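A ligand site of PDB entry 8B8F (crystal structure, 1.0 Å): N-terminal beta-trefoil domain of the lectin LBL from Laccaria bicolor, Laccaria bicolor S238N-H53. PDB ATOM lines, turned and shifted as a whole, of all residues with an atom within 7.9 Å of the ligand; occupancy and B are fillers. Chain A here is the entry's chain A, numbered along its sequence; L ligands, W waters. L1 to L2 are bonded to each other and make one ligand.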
ATOM      1  N   VAL A  71     -14.756  18.725  -8.836  1.00  0.00           N
ATOM      2  CA  VAL A  71     -14.111  19.830  -9.538  1.00  0.00           C
ATOM      3  C   VAL A  71     -14.802  20.061 -10.876  1.00  0.00           C
ATOM      4  O   VAL A  71     -15.326  19.128 -11.507  1.00  0.00           O
ATOM      5  CB  VAL A  71     -12.579  19.627  -9.729  1.00  0.00           C
ATOM      6  CG1 VAL A  71     -11.871  19.589  -8.390  1.00  0.00           C
ATOM      7  CG2 VAL A  71     -12.287  18.382 -10.550  1.00  0.00           C
ATOM      8  N   LEU A  72     -14.782  21.317 -11.337  1.00  0.00           N
ATOM      9  CA  LEU A  72     -15.347  21.637 -12.639  1.00  0.00           C
ATOM     10  C   LEU A  72     -14.448  21.101 -13.757  1.00  0.00           C
ATOM     11  O   LEU A  72     -13.229  20.969 -13.607  1.00  0.00           O
ATOM     12  CB  LEU A  72     -15.498  23.146 -12.791  1.00  0.00           C
ATOM     13  CG  LEU A  72     -16.425  23.853 -11.778  1.00  0.00           C
ATOM     14  CD1 LEU A  72     -16.549  25.338 -12.128  1.00  0.00           C
ATOM     15  CD2 LEU A  72     -17.776  23.187 -11.716  1.00  0.00           C
ATOM     16  N   PHE A  73     -15.050  20.861 -14.932  1.00  0.00           N
ATOM     17  CA  PHE A  73     -14.300  20.543 -16.125  1.00  0.00           C
ATOM     18  C   PHE A  73     -14.868  21.289 -17.331  1.00  0.00           C
ATOM     19  O   PHE A  73     -16.047  21.680 -17.359  1.00  0.00           O
ATOM     20  CB  PHE A  73     -14.248  19.012 -16.425  1.00  0.00           C
ATOM     21  CG  PHE A  73     -15.571  18.403 -16.873  1.00  0.00           C
ATOM     22  CD1 PHE A  73     -16.015  18.533 -18.179  1.00  0.00           C
ATOM     23  CD2 PHE A  73     -16.323  17.637 -15.999  1.00  0.00           C
ATOM     24  CE1 PHE A  73     -17.207  17.943 -18.592  1.00  0.00           C
ATOM     25  CE2 PHE A  73     -17.508  17.042 -16.406  1.00  0.00           C
ATOM     26  CZ  PHE A  73     -17.953  17.224 -17.699  1.00  0.00           C
ATOM     27  N   SER A  74     -14.024  21.454 -18.343  1.00  0.00           N
ATOM     28  CA  SER A  74     -14.408  22.077 -19.608  1.00  0.00           C
ATOM     29  C   SER A  74     -13.666  21.386 -20.739  1.00  0.00           C
ATOM     30  O   SER A  74     -12.436  21.371 -20.747  1.00  0.00           O
ATOM     31  CB  SER A  74     -14.052  23.561 -19.589  1.00  0.00           C
ATOM     32  OG  SER A  74     -14.411  24.224 -20.793  1.00  0.00           O
ATOM     33  N   ARG A  75     -14.421  20.845 -21.710  1.00  0.00           N
ATOM     34  CA  ARG A  75     -13.886  20.065 -22.829  1.00  0.00           C
ATOM     35  C   ARG A  75     -14.739  20.360 -24.082  1.00  0.00           C
ATOM     36  O   ARG A  75     -15.896  20.766 -24.003  1.00  0.00           O
ATOM     37  CB  ARG A  75     -13.841  18.564 -22.432  1.00  0.00           C
ATOM     38  CG  ARG A  75     -15.214  17.963 -22.274  1.00  0.00           C
ATOM     39  CD  ARG A  75     -15.189  16.617 -21.570  1.00  0.00           C
ATOM     40  NE  ARG A  75     -16.540  16.092 -21.483  1.00  0.00           N
ATOM     41  CZ  ARG A  75     -16.978  15.258 -20.550  1.00  0.00           C
ATOM     42  NH1 ARG A  75     -16.148  14.692 -19.679  1.00  0.00           N
ATOM     43  NH2 ARG A  75     -18.281  14.980 -20.494  1.00  0.00           N
ATOM     44  N   SER A  77     -15.528  17.889 -26.217  1.00  0.00           N
ATOM     45  CA  SER A  77     -16.270  16.641 -26.376  1.00  0.00           C
ATOM     46  C   SER A  77     -15.685  15.635 -25.382  1.00  0.00           C
ATOM     47  O   SER A  77     -14.528  15.784 -24.957  1.00  0.00           O
ATOM     48  CB  SER A  77     -16.107  16.095 -27.800  1.00  0.00           C
ATOM     49  OG  SER A  77     -14.807  15.575 -27.941  1.00  0.00           O
ATOM     50  N   PRO A  78     -16.454  14.610 -24.968  1.00  0.00           N
ATOM     51  CA  PRO A  78     -17.853  14.382 -25.306  1.00  0.00           C
ATOM     52  C   PRO A  78     -18.745  15.390 -24.595  1.00  0.00           C
ATOM     53  O   PRO A  78     -18.283  16.222 -23.807  1.00  0.00           O
ATOM     54  CB  PRO A  78     -18.114  12.971 -24.773  1.00  0.00           C
ATOM     55  CG  PRO A  78     -17.166  12.813 -23.660  1.00  0.00           C
ATOM     56  CD  PRO A  78     -15.934  13.559 -24.082  1.00  0.00           C
ATOM     57  N   ASP A  79     -20.032  15.300 -24.888  1.00  0.00           N
ATOM     58  CA  ASP A  79     -21.033  16.019 -24.140  1.00  0.00           C
ATOM     59  C   ASP A  79     -21.270  15.309 -22.815  1.00  0.00           C
ATOM     60  O   ASP A  79     -21.205  14.082 -22.728  1.00  0.00           O
ATOM     61  CB  ASP A  79     -22.353  16.063 -24.914  1.00  0.00           C
ATOM     62  CG  ASP A  79     -22.296  16.980 -26.128  1.00  0.00           C
ATOM     63  OD1 ASP A  79     -21.662  18.050 -26.068  1.00  0.00           O
ATOM     64  OD2 ASP A  79     -22.930  16.654 -27.146  1.00  0.00           O
ATOM     65  N   PRO A  80     -21.578  16.074 -21.752  1.00  0.00           N
ATOM     66  CA  PRO A  80     -21.648  17.532 -21.731  1.00  0.00           C
ATOM     67  C   PRO A  80     -20.261  18.166 -21.757  1.00  0.00           C
ATOM     68  O   PRO A  80     -19.295  17.623 -21.201  1.00  0.00           O
ATOM     69  CB  PRO A  80     -22.347  17.811 -20.389  1.00  0.00           C
ATOM     70  CG  PRO A  80     -21.986  16.672 -19.522  1.00  0.00           C
ATOM     71  CD  PRO A  80     -21.896  15.482 -20.441  1.00  0.00           C
ATOM     72  N   ARG A  81     -20.155  19.323 -22.409  1.00  0.00           N
ATOM     73  CA  ARG A  81     -18.859  19.999 -22.522  1.00  0.00           C
ATOM     74  C   ARG A  81     -18.404  20.639 -21.215  1.00  0.00           C
ATOM     75  O   ARG A  81     -17.195  20.823 -21.011  1.00  0.00           O
ATOM     76  CB  ARG A  81     -18.937  21.023 -23.640  1.00  0.00           C
ATOM     77  CG  ARG A  81     -19.032  20.375 -25.014  1.00  0.00           C
ATOM     78  CD  ARG A  81     -19.822  21.224 -25.974  1.00  0.00           C
ATOM     79  NE  ARG A  81     -19.277  22.559 -26.075  1.00  0.00           N
ATOM     80  CZ  ARG A  81     -19.654  23.441 -26.986  1.00  0.00           C
ATOM     81  NH1 ARG A  81     -20.594  23.151 -27.869  1.00  0.00           N
ATOM     82  NH2 ARG A  81     -19.072  24.636 -27.014  1.00  0.00           N
ATOM     83  N   VAL A  82     -19.348  20.992 -20.330  1.00  0.00           N
ATOM     84  CA  VAL A  82     -19.031  21.604 -19.044  1.00  0.00           C
ATOM     85  C   VAL A  82     -19.761  20.808 -17.968  1.00  0.00           C
ATOM     86  O   VAL A  82     -20.957  20.493 -18.118  1.00  0.00           O
ATOM     87  CB  VAL A  82     -19.421  23.104 -18.999  1.00  0.00           C
ATOM     88  CG1 VAL A  82     -19.262  23.697 -17.587  1.00  0.00           C
ATOM     89  CG2 VAL A  82     -18.583  23.858 -20.002  1.00  0.00           C
ATOM     90  N   GLY A  83     -19.080  20.508 -16.881  1.00  0.00           N
ATOM     91  CA  GLY A  83     -19.689  19.731 -15.827  1.00  0.00           C
ATOM     92  C   GLY A  83     -18.759  19.636 -14.641  1.00  0.00           C
ATOM     93  O   GLY A  83     -17.906  20.517 -14.451  1.00  0.00           O
ATOM     94  N   HIS A  84     -18.949  18.592 -13.840  1.00  0.00           N
ATOM     95  CA  HIS A  84     -18.137  18.386 -12.652  1.00  0.00           C
ATOM     96  C   HIS A  84     -17.810  16.900 -12.504  1.00  0.00           C
ATOM     97  O   HIS A  84     -18.509  16.042 -13.061  1.00  0.00           O
ATOM     98  CB  HIS A  84     -18.762  18.984 -11.370  1.00  0.00           C
ATOM     99  CG  HIS A  84     -20.107  18.450 -10.998  1.00  0.00           C
ATOM    100  ND1 HIS A  84     -20.827  18.998  -9.965  1.00  0.00           N
ATOM    101  CD2 HIS A  84     -20.871  17.450 -11.532  1.00  0.00           C
ATOM    102  CE1 HIS A  84     -21.978  18.348  -9.888  1.00  0.00           C
ATOM    103  NE2 HIS A  84     -22.024  17.400 -10.809  1.00  0.00           N
ATOM    104  N   ILE A  85     -16.743  16.600 -11.769  1.00  0.00           N
ATOM    105  CA  ILE A  85     -16.313  15.209 -11.576  1.00  0.00           C
ATOM    106  C   ILE A  85     -15.541  15.093 -10.251  1.00  0.00           C
ATOM    107  O   ILE A  85     -14.903  16.046  -9.799  1.00  0.00           O
ATOM    108  CB  ILE A  85     -15.458  14.728 -12.783  1.00  0.00           C
ATOM    109  CG1 ILE A  85     -15.365  13.186 -12.802  1.00  0.00           C
ATOM    110  CG2 ILE A  85     -14.084  15.412 -12.802  1.00  0.00           C
ATOM    111  CD1 ILE A  85     -15.029  12.595 -14.139  1.00  0.00           C
ATOM    112  N   ASP A  86     -15.617  13.913  -9.633  1.00  0.00           N
ATOM    113  CA  ASP A  86     -14.905  13.683  -8.382  1.00  0.00           C
ATOM    114  C   ASP A  86     -13.396  13.861  -8.532  1.00  0.00           C
ATOM    115  O   ASP A  86     -12.813  13.674  -9.610  1.00  0.00           O
ATOM    116  CB  ASP A  86     -15.213  12.272  -7.853  1.00  0.00           C
ATOM    117  CG  ASP A  86     -16.597  12.156  -7.191  1.00  0.00           C
ATOM    118  OD1 ASP A  86     -17.349  13.149  -7.115  1.00  0.00           O
ATOM    119  OD2 ASP A  86     -16.934  11.033  -6.745  1.00  0.00           O
ATOM    120  N   GLY A  89      -8.715  17.226  -9.222  1.00  0.00           N
ATOM    121  CA  GLY A  89      -8.057  17.585 -10.460  1.00  0.00           C
ATOM    122  C   GLY A  89      -7.277  16.445 -11.092  1.00  0.00           C
ATOM    123  O   GLY A  89      -6.139  16.622 -11.555  1.00  0.00           O
ATOM    124  N   LYS A  90      -7.878  15.258 -11.155  1.00  0.00           N
ATOM    125  CA  LYS A  90      -7.236  14.086 -11.744  1.00  0.00           C
ATOM    126  C   LYS A  90      -7.092  14.157 -13.255  1.00  0.00           C
ATOM    127  O   LYS A  90      -6.253  13.431 -13.799  1.00  0.00           O
ATOM    128  CB  LYS A  90      -8.048  12.805 -11.430  1.00  0.00           C
ATOM    129  CG  LYS A  90      -8.180  12.531  -9.959  1.00  0.00           C
ATOM    130  CD  LYS A  90      -8.859  11.244  -9.649  1.00  0.00           C
ATOM    131  CE  LYS A  90     -10.260  11.223 -10.168  1.00  0.00           C
ATOM    132  NZ  LYS A  90     -10.950   9.962  -9.725  1.00  0.00           N
ATOM    133  N   TYR A  91      -7.949  14.943 -13.940  1.00  0.00           N
ATOM    134  CA  TYR A  91      -8.023  14.970 -15.389  1.00  0.00           C
ATOM    135  C   TYR A  91      -7.497  16.293 -15.947  1.00  0.00           C
ATOM    136  O   TYR A  91      -7.673  17.336 -15.303  1.00  0.00           O
ATOM    137  CB  TYR A  91      -9.467  14.787 -15.874  1.00  0.00           C
ATOM    138  CG  TYR A  91     -10.102  13.483 -15.441  1.00  0.00           C
ATOM    139  CD1 TYR A  91      -9.935  12.322 -16.162  1.00  0.00           C
ATOM    140  CD2 TYR A  91     -10.849  13.449 -14.277  1.00  0.00           C
ATOM    141  CE1 TYR A  91     -10.521  11.145 -15.731  1.00  0.00           C
ATOM    142  CE2 TYR A  91     -11.432  12.295 -13.829  1.00  0.00           C
ATOM    143  CZ  TYR A  91     -11.276  11.143 -14.549  1.00  0.00           C
ATOM    144  OH  TYR A  91     -11.885  10.020 -14.031  1.00  0.00           O
ATOM    145  N   PRO A  92      -6.901  16.298 -17.152  1.00  0.00           N
ATOM    146  CA  PRO A  92      -6.352  17.577 -17.689  1.00  0.00           C
ATOM    147  C   PRO A  92      -7.381  18.692 -17.811  1.00  0.00           C
ATOM    148  O   PRO A  92      -7.060  19.867 -17.563  1.00  0.00           O
ATOM    149  CB  PRO A  92      -5.774  17.178 -19.064  1.00  0.00           C
ATOM    150  CG  PRO A  92      -5.457  15.754 -18.936  1.00  0.00           C
ATOM    151  CD  PRO A  92      -6.480  15.155 -17.977  1.00  0.00           C
ATOM    152  N   ASP A  93      -8.599  18.356 -18.190  1.00  0.00           N
ATOM    153  CA  ASP A  93      -9.630  19.362 -18.391  1.00  0.00           C
ATOM    154  C   ASP A  93     -10.235  19.891 -17.090  1.00  0.00           C
ATOM    155  O   ASP A  93     -11.211  20.647 -17.133  1.00  0.00           O
ATOM    156  CB  ASP A  93     -10.697  18.858 -19.368  1.00  0.00           C
ATOM    157  CG  ASP A  93     -11.484  17.673 -18.843  1.00  0.00           C
ATOM    158  OD1 ASP A  93     -11.315  17.323 -17.656  1.00  0.00           O
ATOM    159  OD2 ASP A  93     -12.278  17.089 -19.630  1.00  0.00           O
ATOM    160  N   ASN A  94      -9.604  19.565 -15.959  1.00  0.00           N
ATOM    161  CA  ASN A  94      -9.926  20.160 -14.666  1.00  0.00           C
ATOM    162  C   ASN A  94      -9.055  21.367 -14.322  1.00  0.00           C
ATOM    163  O   ASN A  94      -9.269  21.991 -13.278  1.00  0.00           O
ATOM    164  CB  ASN A  94      -9.737  19.133 -13.529  1.00  0.00           C
ATOM    165  CG  ASN A  94     -10.529  17.834 -13.632  1.00  0.00           C
ATOM    166  OD1 ASN A  94     -10.211  16.868 -12.920  1.00  0.00           O
ATOM    167  ND2 ASN A  94     -11.562  17.774 -14.486  1.00  0.00           N
ATOM    168  N   TRP A  95      -8.061  21.698 -15.155  1.00  0.00           N
ATOM    169  CA  TRP A  95      -7.052  22.688 -14.807  1.00  0.00           C
ATOM    170  C   TRP A  95      -7.286  23.977 -15.586  1.00  0.00           C
ATOM    171  O   TRP A  95      -7.237  24.007 -16.823  1.00  0.00           O
ATOM    172  CB  TRP A  95      -5.638  22.117 -15.005  1.00  0.00           C
ATOM    173  CG  TRP A  95      -5.430  21.068 -13.972  1.00  0.00           C
ATOM    174  CD1 TRP A  95      -5.617  19.724 -14.087  1.00  0.00           C
ATOM    175  CD2 TRP A  95      -5.128  21.311 -12.580  1.00  0.00           C
ATOM    176  NE1 TRP A  95      -5.444  19.108 -12.855  1.00  0.00           N
ATOM    177  CE2 TRP A  95      -5.164  20.070 -11.923  1.00  0.00           C
ATOM    178  CE3 TRP A  95      -4.887  22.457 -11.829  1.00  0.00           C
ATOM    179  CZ2 TRP A  95      -4.933  19.956 -10.540  1.00  0.00           C
ATOM    180  CZ3 TRP A  95      -4.675  22.335 -10.467  1.00  0.00           C
ATOM    181  CH2 TRP A  95      -4.713  21.097  -9.838  1.00  0.00           C
HETATM  182  C1  LIG L   1     -19.577   9.989 -17.089  1.00  0.00           C
HETATM  183  C2  LIG L   1     -19.428  11.510 -17.014  1.00  0.00           C
HETATM  184  C3  LIG L   1     -18.300  12.019 -17.906  1.00  0.00           C
HETATM  185  C4  LIG L   1     -17.010  11.224 -17.630  1.00  0.00           C
HETATM  186  C5  LIG L   1     -17.290   9.719 -17.693  1.00  0.00           C
HETATM  187  C6  LIG L   1     -16.068   8.869 -17.296  1.00  0.00           C
HETATM  188  O1  LIG L   1     -20.088   9.625 -18.330  1.00  0.00           O
HETATM  189  O2  LIG L   1     -20.657  12.053 -17.391  1.00  0.00           O
HETATM  190  O3  LIG L   1     -18.088  13.404 -17.731  1.00  0.00           O
HETATM  191  O4  LIG L   1     -16.066  11.540 -18.624  1.00  0.00           O
HETATM  192  O5  LIG L   1     -18.345   9.373 -16.829  1.00  0.00           O
HETATM  193  O6  LIG L   1     -15.592   9.261 -16.028  1.00  0.00           O
HETATM  194  C1  LG2 L   2     -14.767  11.883 -18.186  1.00  0.00           C
HETATM  195  C2  LG2 L   2     -13.859  11.827 -19.424  1.00  0.00           C
HETATM  196  C3  LG2 L   2     -12.478  12.448 -19.123  1.00  0.00           C
HETATM  197  C4  LG2 L   2     -12.656  13.859 -18.520  1.00  0.00           C
HETATM  198  C5  LG2 L   2     -13.583  13.749 -17.293  1.00  0.00           C
HETATM  199  C6  LG2 L   2     -13.913  15.101 -16.657  1.00  0.00           C
HETATM  200  O1  LG2 L   2     -13.717  10.492 -19.908  1.00  0.00           O
HETATM  201  O2  LG2 L   2     -11.673  12.486 -20.291  1.00  0.00           O
HETATM  202  O3  LG2 L   2     -13.239  14.694 -19.499  1.00  0.00           O
HETATM  203  O4  LG2 L   2     -14.832  13.179 -17.663  1.00  0.00           O
HETATM  204  O5  LG2 L   2     -12.777  15.728 -16.106  1.00  0.00           O
HETATM  205  O   HOH W   1     -20.477  12.152 -20.810  1.00  0.00           O
HETATM  206  O   HOH W   2     -22.506  11.768 -19.093  1.00  0.00           O
HETATM  207  O   HOH W   3     -12.848   8.278 -15.520  1.00  0.00           O
HETATM  208  O   HOH W   4     -20.662  14.986 -17.085  1.00  0.00           O
HETATM  209  O   HOH W   5     -14.381   9.052 -13.278  1.00  0.00           O
HETATM  210  O   HOH W   6     -23.416  13.931 -17.680  1.00  0.00           O
HETATM  211  O   HOH W   7     -11.311  16.239 -21.908  1.00  0.00           O
HETATM  212  O   HOH W   8     -18.518  13.858 -14.924  1.00  0.00           O
HETATM  213  O   HOH W   9      -9.015  13.226 -19.627  1.00  0.00           O
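The side-chain carboxylate of Asp 93 is in hydrogen-bond range of an oxygen (O3) of LG2 L2, 2.6 Å away.
O4 of LG2 L2 lies within hydrogen-bond range of NH1 of Arg 75, 2.8 Å away.
An oxygen (O5) of LG2 L2 sits at hydrogen-bond distance from the side-chain amide nitrogen of Asn 94 (2.9 Å).
The side-chain amide nitrogen of Asn 94 is in hydrogen-bond range of the side-chain carboxylate of Asp 93, 3.2 Å away.
N of Ser 74 is in hydrogen-bond range of O of Asp 93 (3.2 Å).
The guanidinium group (NH2) of Arg 75 lies within hydrogen-bond range of the backbone carbonyl oxygen (O) of Pro 80 (2.9 Å).
The backbone NH (N) of Arg 75 lies within hydrogen-bond range of the backbone carbonyl oxygen (O) of Arg 81 (2.9 Å).
The side-chain amide oxygen (OD1) of Asn 94 sits at hydrogen-bond distance from the backbone NH (N) of Tyr 91, 3.1 Å away.
The side-chain amide oxygen (OD1) of Asn 94 is in hydrogen-bond range of the backbone NH (N) of Lys 90 (3.3 Å).
The backbone NH of Phe 73 sits at hydrogen-bond distance from the backbone carbonyl oxygen of Gly 83 (2.9 Å).
O of Ile 85 lies within hydrogen-bond range of N of Val 71 (2.9 Å).
CD2 of Phe 73 touches C6 of LG2 L2, 3.6 Å away.
Ile 85 touches the ligand.
CB of Tyr 91 touches O5 of LG2 L2 (3.4 Å).
Of the 22 residues printed, 6 come within 4 Å of the ligand.
Water W8 bridges O of His 84 and O3 of LIG L1.
Water W3 bridges OH of Tyr 91 and O6 of LIG L1.
Water W5 bridges the side-chain hydroxyl (OH) of Tyr 91 (2.8 Å) and an oxygen (O6) of LIG L1 (3.0 Å).
Water W1 lies within hydrogen-bond range of O of Asp 79 (2.8 Å) and O2 of LIG L1 (3.4 Å).
Water W7 lies within hydrogen-bond range of the side-chain carboxylate of Asp 93 (2.6 Å) and an oxygen (O3) of LG2 L2 (3.5 Å).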
